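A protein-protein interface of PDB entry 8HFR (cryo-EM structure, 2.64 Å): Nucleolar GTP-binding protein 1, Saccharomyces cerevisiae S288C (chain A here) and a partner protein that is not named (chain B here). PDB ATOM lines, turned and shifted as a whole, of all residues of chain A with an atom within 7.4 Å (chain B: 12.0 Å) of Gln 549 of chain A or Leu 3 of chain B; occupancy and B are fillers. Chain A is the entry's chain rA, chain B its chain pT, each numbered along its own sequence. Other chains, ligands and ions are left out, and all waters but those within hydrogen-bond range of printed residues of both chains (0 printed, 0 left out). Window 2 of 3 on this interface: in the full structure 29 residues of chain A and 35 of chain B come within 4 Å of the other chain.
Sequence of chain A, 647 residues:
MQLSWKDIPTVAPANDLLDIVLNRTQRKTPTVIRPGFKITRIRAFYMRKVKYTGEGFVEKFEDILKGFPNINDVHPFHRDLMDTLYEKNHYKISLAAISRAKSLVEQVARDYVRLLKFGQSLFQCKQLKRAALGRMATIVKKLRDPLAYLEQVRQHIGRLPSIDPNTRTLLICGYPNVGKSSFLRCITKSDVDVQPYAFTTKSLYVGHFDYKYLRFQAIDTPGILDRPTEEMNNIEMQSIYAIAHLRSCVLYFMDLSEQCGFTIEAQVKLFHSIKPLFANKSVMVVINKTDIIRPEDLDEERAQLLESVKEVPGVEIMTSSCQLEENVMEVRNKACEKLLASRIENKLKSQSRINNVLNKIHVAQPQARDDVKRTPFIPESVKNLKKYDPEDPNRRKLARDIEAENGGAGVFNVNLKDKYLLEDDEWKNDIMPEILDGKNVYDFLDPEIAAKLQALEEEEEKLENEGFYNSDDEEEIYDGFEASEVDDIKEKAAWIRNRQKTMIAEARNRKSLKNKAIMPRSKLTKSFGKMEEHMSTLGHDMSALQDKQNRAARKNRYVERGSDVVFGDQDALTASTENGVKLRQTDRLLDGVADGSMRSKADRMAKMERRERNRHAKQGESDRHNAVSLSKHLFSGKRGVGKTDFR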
ATOM      1  N   THR A 525     -13.646  -0.321   9.695  1.00  0.00           N
ATOM      2  CA  THR A 525     -13.320  -1.735   9.622  1.00  0.00           C
ATOM      3  C   THR A 525     -11.822  -1.881   9.398  1.00  0.00           C
ATOM      4  O   THR A 525     -11.189  -1.014   8.794  1.00  0.00           O
ATOM      5  CB  THR A 525     -14.123  -2.449   8.519  1.00  0.00           C
ATOM      6  OG1 THR A 525     -13.752  -3.832   8.466  1.00  0.00           O
ATOM      7  CG2 THR A 525     -13.908  -1.808   7.153  1.00  0.00           C
ATOM      8  N   SER A 527      -8.346  -4.925   8.962  1.00  0.00           N
ATOM      9  CA  SER A 527      -7.973  -6.106   8.199  1.00  0.00           C
ATOM     10  C   SER A 527      -7.369  -7.177   9.099  1.00  0.00           C
ATOM     11  O   SER A 527      -6.740  -6.883  10.126  1.00  0.00           O
ATOM     12  CB  SER A 527      -6.977  -5.751   7.095  1.00  0.00           C
ATOM     13  OG  SER A 527      -7.429  -4.644   6.340  1.00  0.00           O
ATOM     14  N   PHE A 528      -7.555  -8.431   8.678  1.00  0.00           N
ATOM     15  CA  PHE A 528      -7.081  -9.564   9.461  1.00  0.00           C
ATOM     16  C   PHE A 528      -5.563  -9.621   9.517  1.00  0.00           C
ATOM     17  O   PHE A 528      -5.010 -10.125  10.497  1.00  0.00           O
ATOM     18  CB  PHE A 528      -7.631 -10.874   8.901  1.00  0.00           C
ATOM     19  CG  PHE A 528      -7.359 -12.060   9.778  1.00  0.00           C
ATOM     20  CD1 PHE A 528      -8.168 -12.326  10.863  1.00  0.00           C
ATOM     21  CD2 PHE A 528      -6.288 -12.900   9.527  1.00  0.00           C
ATOM     22  CE1 PHE A 528      -7.918 -13.408  11.676  1.00  0.00           C
ATOM     23  CE2 PHE A 528      -6.033 -13.979  10.343  1.00  0.00           C
ATOM     24  CZ  PHE A 528      -6.850 -14.232  11.414  1.00  0.00           C
ATOM     25  N   GLY A 529      -4.876  -9.119   8.490  1.00  0.00           N
ATOM     26  CA  GLY A 529      -3.422  -9.110   8.521  1.00  0.00           C
ATOM     27  C   GLY A 529      -2.871  -8.208   9.608  1.00  0.00           C
ATOM     28  O   GLY A 529      -1.949  -8.582  10.337  1.00  0.00           O
ATOM     29  N   MET A 531      -4.620  -7.326  12.246  1.00  0.00           N
ATOM     30  CA  MET A 531      -5.038  -7.981  13.486  1.00  0.00           C
ATOM     31  C   MET A 531      -4.052  -9.060  13.912  1.00  0.00           C
ATOM     32  O   MET A 531      -3.656  -9.130  15.080  1.00  0.00           O
ATOM     33  CB  MET A 531      -6.431  -8.579  13.313  1.00  0.00           C
ATOM     34  CG  MET A 531      -7.073  -8.995  14.612  1.00  0.00           C
ATOM     35  SD  MET A 531      -8.729  -9.634  14.364  1.00  0.00           S
ATOM     36  CE  MET A 531      -9.209  -9.957  16.047  1.00  0.00           C
ATOM     37  N   SER A 543      -4.641 -19.644  16.713  1.00  0.00           N
ATOM     38  CA  SER A 543      -5.229 -20.840  16.118  1.00  0.00           C
ATOM     39  C   SER A 543      -6.736 -20.684  15.930  1.00  0.00           C
ATOM     40  O   SER A 543      -7.267 -20.959  14.846  1.00  0.00           O
ATOM     41  CB  SER A 543      -4.901 -22.059  16.979  1.00  0.00           C
ATOM     42  OG  SER A 543      -5.044 -21.756  18.350  1.00  0.00           O
ATOM     43  N   ALA A 544      -7.435 -20.200  16.964  1.00  0.00           N
ATOM     44  CA  ALA A 544      -8.877 -19.992  16.867  1.00  0.00           C
ATOM     45  C   ALA A 544      -9.220 -18.857  15.907  1.00  0.00           C
ATOM     46  O   ALA A 544     -10.182 -18.957  15.133  1.00  0.00           O
ATOM     47  CB  ALA A 544      -9.451 -19.720  18.255  1.00  0.00           C
ATOM     48  N   LEU A 545      -8.421 -17.787  15.918  1.00  0.00           N
ATOM     49  CA  LEU A 545      -8.640 -16.673  15.002  1.00  0.00           C
ATOM     50  C   LEU A 545      -8.362 -17.071  13.556  1.00  0.00           C
ATOM     51  O   LEU A 545      -9.095 -16.669  12.642  1.00  0.00           O
ATOM     52  CB  LEU A 545      -7.765 -15.493  15.417  1.00  0.00           C
ATOM     53  CG  LEU A 545      -8.408 -14.365  16.225  1.00  0.00           C
ATOM     54  CD1 LEU A 545      -9.047 -14.862  17.489  1.00  0.00           C
ATOM     55  CD2 LEU A 545      -7.346 -13.344  16.567  1.00  0.00           C
ATOM     56  N   GLN A 546      -7.331 -17.887  13.335  1.00  0.00           N
ATOM     57  CA  GLN A 546      -7.033 -18.365  11.992  1.00  0.00           C
ATOM     58  C   GLN A 546      -8.112 -19.328  11.499  1.00  0.00           C
ATOM     59  O   GLN A 546      -8.443 -19.345  10.307  1.00  0.00           O
ATOM     60  CB  GLN A 546      -5.659 -19.026  11.982  1.00  0.00           C
ATOM     61  CG  GLN A 546      -5.087 -19.266  10.610  1.00  0.00           C
ATOM     62  CD  GLN A 546      -4.921 -17.994   9.823  1.00  0.00           C
ATOM     63  OE1 GLN A 546      -5.744 -17.668   8.972  1.00  0.00           O
ATOM     64  NE2 GLN A 546      -3.847 -17.265  10.095  1.00  0.00           N
ATOM     65  N   ASP A 547      -8.708 -20.094  12.417  1.00  0.00           N
ATOM     66  CA  ASP A 547      -9.835 -20.954  12.068  1.00  0.00           C
ATOM     67  C   ASP A 547     -11.061 -20.148  11.645  1.00  0.00           C
ATOM     68  O   ASP A 547     -11.723 -20.487  10.651  1.00  0.00           O
ATOM     69  CB  ASP A 547     -10.176 -21.850  13.251  1.00  0.00           C
ATOM     70  CG  ASP A 547     -10.976 -23.063  12.850  1.00  0.00           C
ATOM     71  OD1 ASP A 547     -10.597 -23.721  11.861  1.00  0.00           O
ATOM     72  OD2 ASP A 547     -11.981 -23.363  13.532  1.00  0.00           O
ATOM     73  N   LYS A 548     -11.379 -19.076  12.384  1.00  0.00           N
ATOM     74  CA  LYS A 548     -12.524 -18.241  12.015  1.00  0.00           C
ATOM     75  C   LYS A 548     -12.283 -17.507  10.697  1.00  0.00           C
ATOM     76  O   LYS A 548     -13.211 -17.338   9.888  1.00  0.00           O
ATOM     77  CB  LYS A 548     -12.836 -17.239  13.122  1.00  0.00           C
ATOM     78  CG  LYS A 548     -13.173 -17.862  14.453  1.00  0.00           C
ATOM     79  CD  LYS A 548     -14.632 -18.210  14.565  1.00  0.00           C
ATOM     80  CE  LYS A 548     -14.967 -18.614  15.981  1.00  0.00           C
ATOM     81  NZ  LYS A 548     -13.826 -19.302  16.635  1.00  0.00           N
ATOM     82  N   GLN A 549     -11.038 -17.097  10.447  1.00  0.00           N
ATOM     83  CA  GLN A 549     -10.726 -16.450   9.176  1.00  0.00           C
ATOM     84  C   GLN A 549     -10.809 -17.430   8.013  1.00  0.00           C
ATOM     85  O   GLN A 549     -11.235 -17.056   6.913  1.00  0.00           O
ATOM     86  CB  GLN A 549      -9.346 -15.809   9.236  1.00  0.00           C
ATOM     87  CG  GLN A 549      -9.145 -14.751   8.193  1.00  0.00           C
ATOM     88  CD  GLN A 549      -8.319 -15.236   7.048  1.00  0.00           C
ATOM     89  OE1 GLN A 549      -7.371 -15.985   7.240  1.00  0.00           O
ATOM     90  NE2 GLN A 549      -8.671 -14.820   5.843  1.00  0.00           N
ATOM     91  N   ASN A 550     -10.428 -18.690   8.241  1.00  0.00           N
ATOM     92  CA  ASN A 550     -10.576 -19.708   7.203  1.00  0.00           C
ATOM     93  C   ASN A 550     -12.041 -19.995   6.915  1.00  0.00           C
ATOM     94  O   ASN A 550     -12.418 -20.240   5.763  1.00  0.00           O
ATOM     95  CB  ASN A 550      -9.859 -20.987   7.615  1.00  0.00           C
ATOM     96  CG  ASN A 550      -8.426 -21.021   7.152  1.00  0.00           C
ATOM     97  OD1 ASN A 550      -7.848 -19.994   6.814  1.00  0.00           O
ATOM     98  ND2 ASN A 550      -7.841 -22.209   7.135  1.00  0.00           N
ATOM     99  N   ARG A 551     -12.885 -19.953   7.950  1.00  0.00           N
ATOM    100  CA  ARG A 551     -14.323 -20.121   7.753  1.00  0.00           C
ATOM    101  C   ARG A 551     -14.910 -18.993   6.913  1.00  0.00           C
ATOM    102  O   ARG A 551     -15.719 -19.239   6.006  1.00  0.00           O
ATOM    103  CB  ARG A 551     -15.024 -20.191   9.103  1.00  0.00           C
ATOM    104  CG  ARG A 551     -16.240 -21.073   9.126  1.00  0.00           C
ATOM    105  CD  ARG A 551     -16.657 -21.354  10.554  1.00  0.00           C
ATOM    106  NE  ARG A 551     -15.505 -21.644  11.399  1.00  0.00           N
ATOM    107  CZ  ARG A 551     -15.561 -21.775  12.718  1.00  0.00           C
ATOM    108  NH1 ARG A 551     -16.717 -21.642  13.348  1.00  0.00           N
ATOM    109  NH2 ARG A 551     -14.461 -22.041  13.406  1.00  0.00           N
ATOM    110  N   ALA A 552     -14.503 -17.750   7.189  1.00  0.00           N
ATOM    111  CA  ALA A 552     -15.013 -16.617   6.414  1.00  0.00           C
ATOM    112  C   ALA A 552     -14.522 -16.655   4.970  1.00  0.00           C
ATOM    113  O   ALA A 552     -15.271 -16.324   4.038  1.00  0.00           O
ATOM    114  CB  ALA A 552     -14.614 -15.305   7.081  1.00  0.00           C
ATOM    115  N   ALA A 553     -13.272 -17.078   4.763  1.00  0.00           N
ATOM    116  CA  ALA A 553     -12.752 -17.249   3.412  1.00  0.00           C
ATOM    117  C   ALA A 553     -13.434 -18.385   2.658  1.00  0.00           C
ATOM    118  O   ALA A 553     -13.562 -18.309   1.433  1.00  0.00           O
ATOM    119  CB  ALA A 553     -11.250 -17.493   3.462  1.00  0.00           C
ATOM    120  N   ARG A 554     -13.871 -19.432   3.356  1.00  0.00           N
ATOM    121  CA  ARG A 554     -14.629 -20.492   2.700  1.00  0.00           C
ATOM    122  C   ARG A 554     -16.043 -20.031   2.371  1.00  0.00           C
ATOM    123  O   ARG A 554     -16.662 -20.520   1.423  1.00  0.00           O
ATOM    124  CB  ARG A 554     -14.667 -21.740   3.585  1.00  0.00           C
ATOM    125  N   LYS A 555     -16.577 -19.097   3.160  1.00  0.00           N
ATOM    126  CA  LYS A 555     -17.937 -18.637   2.899  1.00  0.00           C
ATOM    127  C   LYS A 555     -17.993 -17.670   1.721  1.00  0.00           C
ATOM    128  O   LYS A 555     -18.904 -17.747   0.890  1.00  0.00           O
ATOM    129  CB  LYS A 555     -18.529 -17.991   4.149  1.00  0.00           C
ATOM    130  CG  LYS A 555     -20.019 -17.733   4.031  1.00  0.00           C
ATOM    131  CD  LYS A 555     -20.638 -17.381   5.364  1.00  0.00           C
ATOM    132  CE  LYS A 555     -22.038 -16.819   5.180  1.00  0.00           C
ATOM    133  NZ  LYS A 555     -23.014 -17.867   4.783  1.00  0.00           N
ATOM    134  N   ASN A 556     -17.031 -16.751   1.625  1.00  0.00           N
ATOM    135  CA  ASN A 556     -17.034 -15.770   0.531  1.00  0.00           C
ATOM    136  C   ASN A 556     -16.357 -16.353  -0.712  1.00  0.00           C
ATOM    137  O   ASN A 556     -15.268 -15.937  -1.112  1.00  0.00           O
ATOM    138  CB  ASN A 556     -16.324 -14.491   0.954  1.00  0.00           C
ATOM    139  CG  ASN A 556     -17.101 -13.693   1.969  1.00  0.00           C
ATOM    140  OD1 ASN A 556     -18.329 -13.651   1.934  1.00  0.00           O
ATOM    141  ND2 ASN A 556     -16.388 -13.035   2.872  1.00  0.00           N
ATOM    142  N   MET B   1     -16.236 -14.939  16.798  1.00  0.00           N
ATOM    143  CA  MET B   1     -16.577 -13.850  15.895  1.00  0.00           C
ATOM    144  C   MET B   1     -16.819 -14.360  14.479  1.00  0.00           C
ATOM    145  O   MET B   1     -16.330 -15.419  14.103  1.00  0.00           O
ATOM    146  CB  MET B   1     -15.463 -12.797  15.892  1.00  0.00           C
ATOM    147  CG  MET B   1     -14.127 -13.326  15.389  1.00  0.00           C
ATOM    148  SD  MET B   1     -12.791 -12.129  15.419  1.00  0.00           S
ATOM    149  CE  MET B   1     -13.575 -10.738  14.629  1.00  0.00           C
ATOM    150  N   ALA B   2     -17.590 -13.608  13.702  1.00  0.00           N
ATOM    151  CA  ALA B   2     -17.697 -13.798  12.262  1.00  0.00           C
ATOM    152  C   ALA B   2     -17.160 -12.544  11.595  1.00  0.00           C
ATOM    153  O   ALA B   2     -17.398 -11.435  12.082  1.00  0.00           O
ATOM    154  CB  ALA B   2     -19.143 -14.057  11.834  1.00  0.00           C
ATOM    155  N   LEU B   3     -16.415 -12.709  10.503  1.00  0.00           N
ATOM    156  CA  LEU B   3     -15.682 -11.547  10.023  1.00  0.00           C
ATOM    157  C   LEU B   3     -16.519 -10.600   9.168  1.00  0.00           C
ATOM    158  O   LEU B   3     -16.962  -9.561   9.671  1.00  0.00           O
ATOM    159  CB  LEU B   3     -14.447 -11.996   9.242  1.00  0.00           C
ATOM    160  CG  LEU B   3     -13.357 -12.822   9.932  1.00  0.00           C
ATOM    161  CD1 LEU B   3     -12.038 -12.609   9.234  1.00  0.00           C
ATOM    162  CD2 LEU B   3     -13.212 -12.498  11.392  1.00  0.00           C
ATOM    163  N   ALA B   4     -16.844 -10.985   7.931  1.00  0.00           N
ATOM    164  CA  ALA B   4     -17.350 -10.016   6.958  1.00  0.00           C
ATOM    165  C   ALA B   4     -17.820 -10.645   5.655  1.00  0.00           C
ATOM    166  O   ALA B   4     -17.760 -11.865   5.479  1.00  0.00           O
ATOM    167  CB  ALA B   4     -16.288  -8.968   6.612  1.00  0.00           C
ATOM    168  N   ILE B   5     -18.267  -9.799   4.729  1.00  0.00           N
ATOM    169  CA  ILE B   5     -18.837 -10.223   3.457  1.00  0.00           C
ATOM    170  C   ILE B   5     -18.668  -9.047   2.495  1.00  0.00           C
ATOM    171  O   ILE B   5     -18.406  -7.921   2.934  1.00  0.00           O
ATOM    172  CB  ILE B   5     -20.309 -10.645   3.647  1.00  0.00           C
ATOM    173  CG1 ILE B   5     -20.797 -11.552   2.516  1.00  0.00           C
ATOM    174  CG2 ILE B   5     -21.211  -9.426   3.769  1.00  0.00           C
ATOM    175  CD1 ILE B   5     -22.098 -12.257   2.827  1.00  0.00           C
ATOM    176  N   SER B   6     -18.782  -9.287   1.182  1.00  0.00           N
ATOM    177  CA  SER B   6     -18.605  -8.211   0.208  1.00  0.00           C
ATOM    178  C   SER B   6     -19.384  -8.431  -1.089  1.00  0.00           C
ATOM    179  O   SER B   6     -20.086  -9.436  -1.241  1.00  0.00           O
ATOM    180  CB  SER B   6     -17.120  -8.026  -0.114  1.00  0.00           C
ATOM    181  OG  SER B   6     -16.432  -7.426   0.971  1.00  0.00           O
ATOM    182  N   HIS B   7     -19.250  -7.493  -2.037  1.00  0.00           N
ATOM    183  CA  HIS B   7     -20.013  -7.462  -3.283  1.00  0.00           C
ATOM    184  C   HIS B   7     -19.173  -7.756  -4.517  1.00  0.00           C
ATOM    185  O   HIS B   7     -19.672  -8.384  -5.459  1.00  0.00           O
ATOM    186  CB  HIS B   7     -20.693  -6.094  -3.449  1.00  0.00           C
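The backbone carbonyl oxygen (O) of Ala 4 of chain B lies within hydrogen-bond range of the side-chain amide nitrogen (ND2) of Asn 556 of chain A (3.2 Å).
Of the 19 printed residues of chain A, 4 touch a printed residue of chain B. Printed residues of chain B that touch a printed residue of chain A: Met 1, Leu 3, Ala 4 and Ile 5. Hydrophobic or aromatic side chains of chain B that line the printed part of chain A: Leu 3 and Ile 5. Among the printed residues, 5 pairs touch across the chains. Among the printed residues, no Asp or Glu carboxylate lies within 4 Å of a Lys or Arg side-chain nitrogen of the other chain.
Among the printed residues, merely in contact across the chains: Asn 556 of chain A with Ile 5 of chain B, Lys 548 of chain A with Met 1 of chain B, Gln 549 of chain A with Leu 3 of chain B and Ala 552 of chain A with Leu 3 of chain B.
Gln 549 of chain A touches just one residue of chain B: Leu 3 (3.7 Å). Of chain A, only Gln 549 (3.7 Å) and Ala 552 (3.96 Å) come within 4 Å of Leu 3 of chain B. No residue of chain B comes within 4 Å of Phe 528 of chain A. No residue of chain B comes within 4 Å of Leu 545 of chain A. No residue of chain B comes within 4 Å of Gln 546 of chain A. Asp 547 of chain A touches none of the printed residues of chain B. Of chain B, only Met 1 comes within 4 Å of Lys 548 of chain A. Arg 551 of chain A touches none of the printed residues of chain B. No residue of chain B comes within 4 Å of Ala 553 of chain A. Of the printed residues of chain A, Ile 5 of chain B touches Asn 556. Of the printed residues of chain B, Asn 556 of chain A touches Ala 4 (3.2 Å) and Ile 5 (3.3 Å). Printed residues of chain A within 4 Å of Met 1 of chain B: Lys 548 (3.3 Å). Printed residues of chain A within 4 Å of Ala 4 of chain B: Asn 556 (3.2 Å). Gly 529 of chain A touches none of the printed residues of chain B. Ser 543 of chain A touches none of the printed residues of chain B. The nearest residue of chain A that does not touch Leu 3 of chain B is Phe 528 of chain A (4.2 Å).
OE1 of Gln 549 of chain A lies close to OE1 of Gln 546 of chain A.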
